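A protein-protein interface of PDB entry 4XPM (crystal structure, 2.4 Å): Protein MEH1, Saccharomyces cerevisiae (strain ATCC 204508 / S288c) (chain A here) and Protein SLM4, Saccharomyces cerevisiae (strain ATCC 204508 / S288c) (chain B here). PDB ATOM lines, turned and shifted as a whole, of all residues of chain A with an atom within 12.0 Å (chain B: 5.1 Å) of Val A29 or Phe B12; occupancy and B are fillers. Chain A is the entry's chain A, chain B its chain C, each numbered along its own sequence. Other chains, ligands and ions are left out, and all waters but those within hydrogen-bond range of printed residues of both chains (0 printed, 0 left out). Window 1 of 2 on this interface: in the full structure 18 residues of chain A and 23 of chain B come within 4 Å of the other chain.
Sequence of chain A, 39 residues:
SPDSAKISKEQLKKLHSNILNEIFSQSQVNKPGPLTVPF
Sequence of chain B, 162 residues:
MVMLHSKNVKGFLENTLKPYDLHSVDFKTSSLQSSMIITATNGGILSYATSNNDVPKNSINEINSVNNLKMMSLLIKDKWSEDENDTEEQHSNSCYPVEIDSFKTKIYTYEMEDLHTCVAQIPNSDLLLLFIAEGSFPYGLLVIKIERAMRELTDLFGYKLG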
ATOM      1  N   ASN A  21      -4.712 -17.073 -31.687  1.00  0.00           N
ATOM      2  CA  ASN A  21      -5.189 -17.085 -30.310  1.00  0.00           C
ATOM      3  C   ASN A  21      -6.302 -16.070 -30.080  1.00  0.00           C
ATOM      4  O   ASN A  21      -7.306 -16.387 -29.444  1.00  0.00           O
ATOM      5  CB  ASN A  21      -4.040 -16.863 -29.305  1.00  0.00           C
ATOM      6  CG  ASN A  21      -3.144 -18.089 -29.150  1.00  0.00           C
ATOM      7  OD1 ASN A  21      -3.525 -19.198 -29.510  1.00  0.00           O
ATOM      8  ND2 ASN A  21      -1.954 -17.892 -28.592  1.00  0.00           N
ATOM      9  N   GLU A  22      -6.129 -14.859 -30.610  1.00  0.00           N
ATOM     10  CA  GLU A  22      -7.110 -13.796 -30.417  1.00  0.00           C
ATOM     11  C   GLU A  22      -8.410 -14.157 -31.110  1.00  0.00           C
ATOM     12  O   GLU A  22      -9.481 -13.995 -30.541  1.00  0.00           O
ATOM     13  CB  GLU A  22      -6.615 -12.454 -30.965  1.00  0.00           C
ATOM     14  CG  GLU A  22      -5.561 -11.746 -30.129  1.00  0.00           C
ATOM     15  CD  GLU A  22      -5.463 -10.247 -30.451  1.00  0.00           C
ATOM     16  OE1 GLU A  22      -4.507  -9.855 -31.150  1.00  0.00           O
ATOM     17  OE2 GLU A  22      -6.340  -9.460 -30.007  1.00  0.00           O
ATOM     18  N   ILE A  23      -8.314 -14.648 -32.341  1.00  0.00           N
ATOM     19  CA  ILE A  23      -9.506 -14.977 -33.116  1.00  0.00           C
ATOM     20  C   ILE A  23     -10.283 -16.106 -32.461  1.00  0.00           C
ATOM     21  O   ILE A  23     -11.501 -16.019 -32.305  1.00  0.00           O
ATOM     22  CB  ILE A  23      -9.154 -15.403 -34.557  1.00  0.00           C
ATOM     23  CG1 ILE A  23      -8.598 -14.222 -35.331  1.00  0.00           C
ATOM     24  CG2 ILE A  23     -10.375 -15.963 -35.276  1.00  0.00           C
ATOM     25  CD1 ILE A  23      -8.124 -14.608 -36.683  1.00  0.00           C
ATOM     26  N   PHE A  24      -9.584 -17.169 -32.071  1.00  0.00           N
ATOM     27  CA  PHE A  24     -10.276 -18.288 -31.430  1.00  0.00           C
ATOM     28  C   PHE A  24     -10.851 -17.897 -30.054  1.00  0.00           C
ATOM     29  O   PHE A  24     -11.946 -18.299 -29.693  1.00  0.00           O
ATOM     30  CB  PHE A  24      -9.382 -19.531 -31.405  1.00  0.00           C
ATOM     31  CG  PHE A  24      -8.982 -20.006 -32.803  1.00  0.00           C
ATOM     32  CD1 PHE A  24      -9.927 -20.082 -33.820  1.00  0.00           C
ATOM     33  CD2 PHE A  24      -7.669 -20.332 -33.108  1.00  0.00           C
ATOM     34  CE1 PHE A  24      -9.573 -20.486 -35.097  1.00  0.00           C
ATOM     35  CE2 PHE A  24      -7.323 -20.740 -34.387  1.00  0.00           C
ATOM     36  CZ  PHE A  24      -8.280 -20.817 -35.379  1.00  0.00           C
ATOM     37  N   SER A  25     -10.139 -17.058 -29.311  1.00  0.00           N
ATOM     38  CA  SER A  25     -10.662 -16.588 -28.038  1.00  0.00           C
ATOM     39  C   SER A  25     -11.952 -15.795 -28.273  1.00  0.00           C
ATOM     40  O   SER A  25     -12.968 -16.039 -27.629  1.00  0.00           O
ATOM     41  CB  SER A  25      -9.621 -15.741 -27.302  1.00  0.00           C
ATOM     42  OG  SER A  25     -10.106 -15.369 -26.032  1.00  0.00           O
ATOM     43  N   GLN A  26     -11.912 -14.876 -29.230  1.00  0.00           N
ATOM     44  CA  GLN A  26     -13.053 -14.021 -29.526  1.00  0.00           C
ATOM     45  C   GLN A  26     -14.160 -14.742 -30.303  1.00  0.00           C
ATOM     46  O   GLN A  26     -15.234 -14.183 -30.532  1.00  0.00           O
ATOM     47  CB  GLN A  26     -12.595 -12.778 -30.282  1.00  0.00           C
ATOM     48  CG  GLN A  26     -11.610 -11.917 -29.492  1.00  0.00           C
ATOM     49  CD  GLN A  26     -11.262 -10.632 -30.209  1.00  0.00           C
ATOM     50  OE1 GLN A  26     -12.005 -10.169 -31.076  1.00  0.00           O
ATOM     51  NE2 GLN A  26     -10.131 -10.041 -29.850  1.00  0.00           N
ATOM     52  N   SER A  27     -13.909 -15.986 -30.694  1.00  0.00           N
ATOM     53  CA  SER A  27     -14.928 -16.763 -31.402  1.00  0.00           C
ATOM     54  C   SER A  27     -15.839 -17.537 -30.463  1.00  0.00           C
ATOM     55  O   SER A  27     -16.772 -18.196 -30.906  1.00  0.00           O
ATOM     56  CB  SER A  27     -14.291 -17.743 -32.372  1.00  0.00           C
ATOM     57  OG  SER A  27     -13.702 -17.060 -33.449  1.00  0.00           O
ATOM     58  N   GLN A  28     -15.554 -17.477 -29.170  1.00  0.00           N
ATOM     59  CA  GLN A  28     -16.361 -18.191 -28.202  1.00  0.00           C
ATOM     60  C   GLN A  28     -17.621 -17.398 -28.012  1.00  0.00           C
ATOM     61  O   GLN A  28     -17.591 -16.173 -27.982  1.00  0.00           O
ATOM     62  CB  GLN A  28     -15.632 -18.309 -26.865  1.00  0.00           C
ATOM     63  CG  GLN A  28     -14.218 -18.878 -26.957  1.00  0.00           C
ATOM     64  CD  GLN A  28     -14.191 -20.393 -27.038  1.00  0.00           C
ATOM     65  OE1 GLN A  28     -14.828 -20.993 -27.907  1.00  0.00           O
ATOM     66  NE2 GLN A  28     -13.452 -21.022 -26.120  1.00  0.00           N
ATOM     67  N   VAL A  29     -18.743 -18.090 -27.916  1.00  0.00           N
ATOM     68  CA  VAL A  29     -19.977 -17.416 -27.548  1.00  0.00           C
ATOM     69  C   VAL A  29     -20.675 -18.195 -26.441  1.00  0.00           C
ATOM     70  O   VAL A  29     -20.707 -19.434 -26.457  1.00  0.00           O
ATOM     71  CB  VAL A  29     -20.888 -17.146 -28.770  1.00  0.00           C
ATOM     72  CG1 VAL A  29     -20.427 -17.931 -29.972  1.00  0.00           C
ATOM     73  CG2 VAL A  29     -22.333 -17.426 -28.443  1.00  0.00           C
ATOM     74  N   ASN A  30     -21.176 -17.468 -25.446  1.00  0.00           N
ATOM     75  CA  ASN A  30     -21.878 -18.111 -24.350  1.00  0.00           C
ATOM     76  C   ASN A  30     -23.335 -18.247 -24.717  1.00  0.00           C
ATOM     77  O   ASN A  30     -23.941 -17.293 -25.209  1.00  0.00           O
ATOM     78  CB  ASN A  30     -21.735 -17.302 -23.059  1.00  0.00           C
ATOM     79  CG  ASN A  30     -20.324 -17.375 -22.468  1.00  0.00           C
ATOM     80  OD1 ASN A  30     -19.643 -18.399 -22.555  1.00  0.00           O
ATOM     81  ND2 ASN A  30     -19.889 -16.283 -21.858  1.00  0.00           N
ATOM     82  N   LYS A  31     -23.901 -19.432 -24.520  1.00  0.00           N
ATOM     83  CA  LYS A  31     -25.360 -19.508 -24.501  1.00  0.00           C
ATOM     84  C   LYS A  31     -25.846 -19.095 -23.113  1.00  0.00           C
ATOM     85  O   LYS A  31     -25.220 -19.422 -22.109  1.00  0.00           O
ATOM     86  CB  LYS A  31     -25.914 -20.878 -24.939  1.00  0.00           C
ATOM     87  CG  LYS A  31     -25.259 -22.087 -24.306  1.00  0.00           C
ATOM     88  CD  LYS A  31     -26.088 -23.337 -24.569  1.00  0.00           C
ATOM     89  CE  LYS A  31     -25.565 -24.513 -23.751  1.00  0.00           C
ATOM     90  NZ  LYS A  31     -26.564 -25.615 -23.655  1.00  0.00           N
ATOM     91  N   PRO A  32     -26.949 -18.340 -23.065  1.00  0.00           N
ATOM     92  CA  PRO A  32     -27.519 -17.856 -21.802  1.00  0.00           C
ATOM     93  C   PRO A  32     -28.141 -18.996 -21.016  1.00  0.00           C
ATOM     94  O   PRO A  32     -28.365 -18.861 -19.816  1.00  0.00           O
ATOM     95  CB  PRO A  32     -28.618 -16.886 -22.260  1.00  0.00           C
ATOM     96  CG  PRO A  32     -28.313 -16.604 -23.724  1.00  0.00           C
ATOM     97  CD  PRO A  32     -27.705 -17.861 -24.233  1.00  0.00           C
ATOM     98  N   GLY A  33     -28.419 -20.103 -21.697  1.00  0.00           N
ATOM     99  CA  GLY A  33     -29.035 -21.262 -21.073  1.00  0.00           C
ATOM    100  C   GLY A  33     -29.342 -22.360 -22.081  1.00  0.00           C
ATOM    101  O   GLY A  33     -28.981 -22.247 -23.252  1.00  0.00           O
ATOM    102  N   PRO A  34     -29.996 -23.441 -21.628  1.00  0.00           N
ATOM    103  CA  PRO A  34     -30.387 -24.524 -22.538  1.00  0.00           C
ATOM    104  C   PRO A  34     -31.280 -23.998 -23.658  1.00  0.00           C
ATOM    105  O   PRO A  34     -32.083 -23.100 -23.414  1.00  0.00           O
ATOM    106  CB  PRO A  34     -31.150 -25.502 -21.629  1.00  0.00           C
ATOM    107  CG  PRO A  34     -31.323 -24.800 -20.319  1.00  0.00           C
ATOM    108  CD  PRO A  34     -30.278 -23.762 -20.220  1.00  0.00           C
ATOM    109  N   LEU A  35     -31.121 -24.538 -24.864  1.00  0.00           N
ATOM    110  CA  LEU A  35     -31.801 -24.016 -26.050  1.00  0.00           C
ATOM    111  C   LEU A  35     -33.042 -24.836 -26.435  1.00  0.00           C
ATOM    112  O   LEU A  35     -33.779 -24.479 -27.357  1.00  0.00           O
ATOM    113  CB  LEU A  35     -30.818 -23.946 -27.225  1.00  0.00           C
ATOM    114  CG  LEU A  35     -29.474 -23.294 -26.877  1.00  0.00           C
ATOM    115  CD1 LEU A  35     -28.496 -23.402 -28.027  1.00  0.00           C
ATOM    116  CD2 LEU A  35     -29.680 -21.835 -26.482  1.00  0.00           C
ATOM    117  N   THR A  36     -33.261 -25.939 -25.725  1.00  0.00           N
ATOM    118  CA  THR A  36     -34.425 -26.787 -25.950  1.00  0.00           C
ATOM    119  C   THR A  36     -35.233 -27.042 -24.676  1.00  0.00           C
ATOM    120  O   THR A  36     -34.701 -27.003 -23.564  1.00  0.00           O
ATOM    121  CB  THR A  36     -34.026 -28.153 -26.521  1.00  0.00           C
ATOM    122  OG1 THR A  36     -33.196 -28.840 -25.578  1.00  0.00           O
ATOM    123  CG2 THR A  36     -33.276 -27.981 -27.813  1.00  0.00           C
ATOM    124  N   LYS B   7     -36.166 -17.523 -25.902  1.00  0.00           N
ATOM    125  CA  LYS B   7     -35.370 -16.459 -25.302  1.00  0.00           C
ATOM    126  C   LYS B   7     -33.865 -16.758 -25.249  1.00  0.00           C
ATOM    127  O   LYS B   7     -33.046 -15.858 -25.473  1.00  0.00           O
ATOM    128  CB  LYS B   7     -35.920 -16.120 -23.908  1.00  0.00           C
ATOM    129  CG  LYS B   7     -34.929 -15.451 -22.975  1.00  0.00           C
ATOM    130  CD  LYS B   7     -35.243 -13.980 -22.783  1.00  0.00           C
ATOM    131  CE  LYS B   7     -35.303 -13.626 -21.305  1.00  0.00           C
ATOM    132  NZ  LYS B   7     -35.778 -12.230 -21.089  1.00  0.00           N
ATOM    133  N   ASN B   8     -33.500 -18.005 -24.955  1.00  0.00           N
ATOM    134  CA  ASN B   8     -32.085 -18.392 -24.936  1.00  0.00           C
ATOM    135  C   ASN B   8     -31.440 -18.540 -26.313  1.00  0.00           C
ATOM    136  O   ASN B   8     -30.250 -18.257 -26.474  1.00  0.00           O
ATOM    137  CB  ASN B   8     -31.849 -19.668 -24.121  1.00  0.00           C
ATOM    138  CG  ASN B   8     -32.095 -19.464 -22.648  1.00  0.00           C
ATOM    139  OD1 ASN B   8     -32.111 -18.334 -22.161  1.00  0.00           O
ATOM    140  ND2 ASN B   8     -32.307 -20.559 -21.927  1.00  0.00           N
ATOM    141  N   VAL B   9     -32.214 -18.991 -27.296  1.00  0.00           N
ATOM    142  CA  VAL B   9     -31.715 -19.065 -28.654  1.00  0.00           C
ATOM    143  C   VAL B   9     -31.479 -17.636 -29.128  1.00  0.00           C
ATOM    144  O   VAL B   9     -30.406 -17.314 -29.628  1.00  0.00           O
ATOM    145  CB  VAL B   9     -32.713 -19.767 -29.584  1.00  0.00           C
ATOM    146  CG1 VAL B   9     -32.343 -19.536 -31.053  1.00  0.00           C
ATOM    147  CG2 VAL B   9     -32.781 -21.248 -29.263  1.00  0.00           C
ATOM    148  N   LYS B  10     -32.487 -16.785 -28.944  1.00  0.00           N
ATOM    149  CA  LYS B  10     -32.379 -15.356 -29.230  1.00  0.00           C
ATOM    150  C   LYS B  10     -31.120 -14.732 -28.593  1.00  0.00           C
ATOM    151  O   LYS B  10     -30.341 -14.048 -29.265  1.00  0.00           O
ATOM    152  CB  LYS B  10     -33.630 -14.642 -28.728  1.00  0.00           C
ATOM    153  CG  LYS B  10     -33.641 -13.117 -28.884  1.00  0.00           C
ATOM    154  CD  LYS B  10     -34.111 -12.715 -30.269  1.00  0.00           C
ATOM    155  CE  LYS B  10     -34.413 -11.219 -30.381  1.00  0.00           C
ATOM    156  NZ  LYS B  10     -34.854 -10.838 -31.774  1.00  0.00           N
ATOM    157  N   GLY B  11     -30.928 -14.970 -27.298  1.00  0.00           N
ATOM    158  CA  GLY B  11     -29.739 -14.507 -26.608  1.00  0.00           C
ATOM    159  C   GLY B  11     -28.454 -15.074 -27.217  1.00  0.00           C
ATOM    160  O   GLY B  11     -27.428 -14.386 -27.328  1.00  0.00           O
ATOM    161  N   PHE B  12     -28.498 -16.336 -27.619  1.00  0.00           N
ATOM    162  CA  PHE B  12     -27.335 -16.917 -28.264  1.00  0.00           C
ATOM    163  C   PHE B  12     -27.000 -16.184 -29.561  1.00  0.00           C
ATOM    164  O   PHE B  12     -25.841 -15.856 -29.808  1.00  0.00           O
ATOM    165  CB  PHE B  12     -27.520 -18.399 -28.540  1.00  0.00           C
ATOM    166  CG  PHE B  12     -26.398 -18.995 -29.345  1.00  0.00           C
ATOM    167  CD1 PHE B  12     -25.257 -19.465 -28.720  1.00  0.00           C
ATOM    168  CD2 PHE B  12     -26.482 -19.074 -30.728  1.00  0.00           C
ATOM    169  CE1 PHE B  12     -24.227 -20.019 -29.461  1.00  0.00           C
ATOM    170  CE2 PHE B  12     -25.459 -19.618 -31.466  1.00  0.00           C
ATOM    171  CZ  PHE B  12     -24.326 -20.092 -30.835  1.00  0.00           C
ATOM    172  N   LEU B  13     -28.016 -15.929 -30.383  1.00  0.00           N
ATOM    173  CA  LEU B  13     -27.793 -15.248 -31.657  1.00  0.00           C
ATOM    174  C   LEU B  13     -27.245 -13.840 -31.432  1.00  0.00           C
ATOM    175  O   LEU B  13     -26.346 -13.394 -32.155  1.00  0.00           O
ATOM    176  CB  LEU B  13     -29.066 -15.229 -32.501  1.00  0.00           C
ATOM    177  CG  LEU B  13     -29.523 -16.632 -32.917  1.00  0.00           C
ATOM    178  CD1 LEU B  13     -30.823 -16.608 -33.735  1.00  0.00           C
ATOM    179  CD2 LEU B  13     -28.401 -17.365 -33.669  1.00  0.00           C
ATOM    180  N   GLU B  14     -27.768 -13.160 -30.411  1.00  0.00           N
ATOM    181  CA  GLU B  14     -27.311 -11.818 -30.085  1.00  0.00           C
ATOM    182  C   GLU B  14     -25.831 -11.811 -29.731  1.00  0.00           C
ATOM    183  O   GLU B  14     -25.116 -10.879 -30.100  1.00  0.00           O
ATOM    184  CB  GLU B  14     -28.184 -11.179 -28.992  1.00  0.00           C
ATOM    185  CG  GLU B  14     -29.573 -10.877 -29.531  1.00  0.00           C
ATOM    186  CD  GLU B  14     -30.503 -10.219 -28.545  1.00  0.00           C
ATOM    187  OE1 GLU B  14     -30.376 -10.470 -27.323  1.00  0.00           O
ATOM    188  OE2 GLU B  14     -31.376  -9.450 -29.010  1.00  0.00           O
ATOM    189  N   ASN B  15     -25.373 -12.865 -29.060  1.00  0.00           N
ATOM    190  CA  ASN B  15     -23.963 -13.011 -28.746  1.00  0.00           C
ATOM    191  C   ASN B  15     -23.093 -13.271 -29.985  1.00  0.00           C
ATOM    192  O   ASN B  15     -21.919 -12.901 -30.008  1.00  0.00           O
ATOM    193  CB  ASN B  15     -23.748 -14.124 -27.719  1.00  0.00           C
ATOM    194  CG  ASN B  15     -24.297 -13.771 -26.350  1.00  0.00           C
ATOM    195  OD1 ASN B  15     -24.374 -12.599 -25.985  1.00  0.00           O
ATOM    196  ND2 ASN B  15     -24.675 -14.786 -25.579  1.00  0.00           N
ATOM    197  N   THR B  16     -23.651 -13.903 -31.015  1.00  0.00           N
ATOM    198  CA  THR B  16     -22.844 -14.223 -32.198  1.00  0.00           C
ATOM    199  C   THR B  16     -22.547 -12.957 -32.983  1.00  0.00           C
ATOM    200  O   THR B  16     -21.715 -12.962 -33.878  1.00  0.00           O
ATOM    201  CB  THR B  16     -23.547 -15.203 -33.148  1.00  0.00           C
ATOM    202  OG1 THR B  16     -24.815 -14.654 -33.534  1.00  0.00           O
ATOM    203  CG2 THR B  16     -23.742 -16.561 -32.492  1.00  0.00           C
ATOM    204  N   LYS B  18     -21.151 -10.142 -32.042  1.00  0.00           N
ATOM    205  CA  LYS B  18     -20.014  -9.323 -31.620  1.00  0.00           C
ATOM    206  C   LYS B  18     -18.889  -9.322 -32.658  1.00  0.00           C
ATOM    207  O   LYS B  18     -18.594 -10.344 -33.270  1.00  0.00           O
ATOM    208  CB  LYS B  18     -19.488  -9.766 -30.244  1.00  0.00           C
ATOM    209  CG  LYS B  18     -18.890 -11.169 -30.229  1.00  0.00           C
ATOM    210  CD  LYS B  18     -18.516 -11.607 -28.817  1.00  0.00           C
ATOM    211  CE  LYS B  18     -17.819 -12.964 -28.845  1.00  0.00           C
ATOM    212  NZ  LYS B  18     -18.523 -13.904 -29.769  1.00  0.00           N
ATOM    213  N   ALA B 149     -19.268 -20.927 -33.436  1.00  0.00           N
ATOM    214  CA  ALA B 149     -20.645 -20.741 -32.968  1.00  0.00           C
ATOM    215  C   ALA B 149     -21.405 -22.069 -32.961  1.00  0.00           C
ATOM    216  O   ALA B 149     -22.067 -22.411 -31.980  1.00  0.00           O
ATOM    217  CB  ALA B 149     -21.378 -19.718 -33.836  1.00  0.00           C
ATOM    218  N   GLU B 152     -21.301 -24.418 -30.109  1.00  0.00           N
ATOM    219  CA  GLU B 152     -22.098 -24.116 -28.923  1.00  0.00           C
ATOM    220  C   GLU B 152     -23.549 -24.555 -29.077  1.00  0.00           C
ATOM    221  O   GLU B 152     -24.366 -24.292 -28.200  1.00  0.00           O
ATOM    222  CB  GLU B 152     -22.064 -22.618 -28.593  1.00  0.00           C
ATOM    223  CG  GLU B 152     -20.728 -21.937 -28.809  1.00  0.00           C
ATOM    224  CD  GLU B 152     -19.668 -22.357 -27.815  1.00  0.00           C
ATOM    225  OE1 GLU B 152     -20.021 -22.976 -26.788  1.00  0.00           O
ATOM    226  OE2 GLU B 152     -18.475 -22.061 -28.065  1.00  0.00           O
ATOM    227  N   LEU B 153     -23.871 -25.215 -30.186  1.00  0.00           N
ATOM    228  CA  LEU B 153     -25.269 -25.531 -30.497  1.00  0.00           C
ATOM    229  C   LEU B 153     -25.573 -27.029 -30.463  1.00  0.00           C
ATOM    230  O   LEU B 153     -26.480 -27.500 -31.148  1.00  0.00           O
ATOM    231  CB  LEU B 153     -25.672 -24.964 -31.863  1.00  0.00           C
ATOM    232  CG  LEU B 153     -25.658 -23.444 -32.016  1.00  0.00           C
ATOM    233  CD1 LEU B 153     -26.114 -23.040 -33.414  1.00  0.00           C
ATOM    234  CD2 LEU B 153     -26.525 -22.788 -30.946  1.00  0.00           C
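The backbone carbonyl oxygen of Gln A26 sits close to the side-chain amino group of Lys B18 (3.4 Å).
O of Gln A28 sits at hydrogen-bond distance from NZ of Lys B18, 3.0 Å away.
The backbone carbonyl oxygen (O) of Asn A30 sits at hydrogen-bond distance from the side-chain amide nitrogen (ND2) of Asn B15, at 2.6 Å.
The backbone carbonyl oxygen (O) of Pro A34 is in hydrogen-bond range of the side-chain amide nitrogen (ND2) of Asn B8, at 3.0 Å.
Of the 14 printed residues of chain B, 8 touch a printed residue of chain A.
Of the 16 printed residues of chain A, 8 touch a printed residue of chain B.
Hydrophobic or aromatic side chains of chain A that line the printed part of chain B: Val A29, Pro A32 and Leu A35.
Among the printed residues, no Asp or Glu carboxylate lies within 4 Å of a Lys or Arg side-chain nitrogen of the other chain.
Of chain A, only Val A29 (3.4 Å) and Pro A32 (3.8 Å) come within 4 Å of Phe B12.
Of chain A, only Leu A35 (3.9 Å) comes within 4 Å of Val B9.
Leu B13 touches none of the printed residues of chain A.
Glu B14 touches none of the printed residues of chain A.
Glu B152 touches just these residues of chain A: Gln A28 and Val A29.
Leu B153 touches just one residue of chain A: Leu A35.
Of the printed residues of chain B, Asn A30 touches Asn B15.
Of the printed residues of chain B, Gln A28 touches Lys B18 (3.0 Å) and Glu B152 (3.8 Å).
Of the printed residues of chain A, Lys B18 touches Gln A26 (3.3 Å) and Gln A28 (3.0 Å).
Printed residues of chain B within 4 Å of Pro A32: Asn B8 (3.4 Å), Gly B11 (3.8 Å) and Phe B12 (3.8 Å).
Lys B7 touches none of the printed residues of chain A.
Phe A24 touches none of the printed residues of chain B.
The nearest printed residue of chain B that does not touch Val A29 is Ala B149 (4.1 Å).
The nearest printed residue of chain B that does not touch Gln A28 is Asn B15 (5.8 Å).
Gln A28 touches Glu B152 (OE1 to OE2, 3.8 Å).
CG2 of Val A29 touches CE1 of Phe B12, at 3.4 Å.
CG2 of Val A29 touches CB of Asn B15, at 3.7 Å.
O of Val A29 touches CD of Glu B152 (3.4 Å).
Pro A32 touches Asn B8 (CD to O, 3.4 Å).
C of Gly B11 touches CG of Pro A32 (3.8 Å).
Pro A32 touches Phe B12.
Leu A35 touches Asn B8.
Leu A35 touches Val B9 (O to CG2, 3.9 Å).
Leu A35 touches Leu B153.
The backbone carbonyl oxygen of Gly B11 sits at hydrogen-bond distance from the side-chain amide nitrogen of Asn B15.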
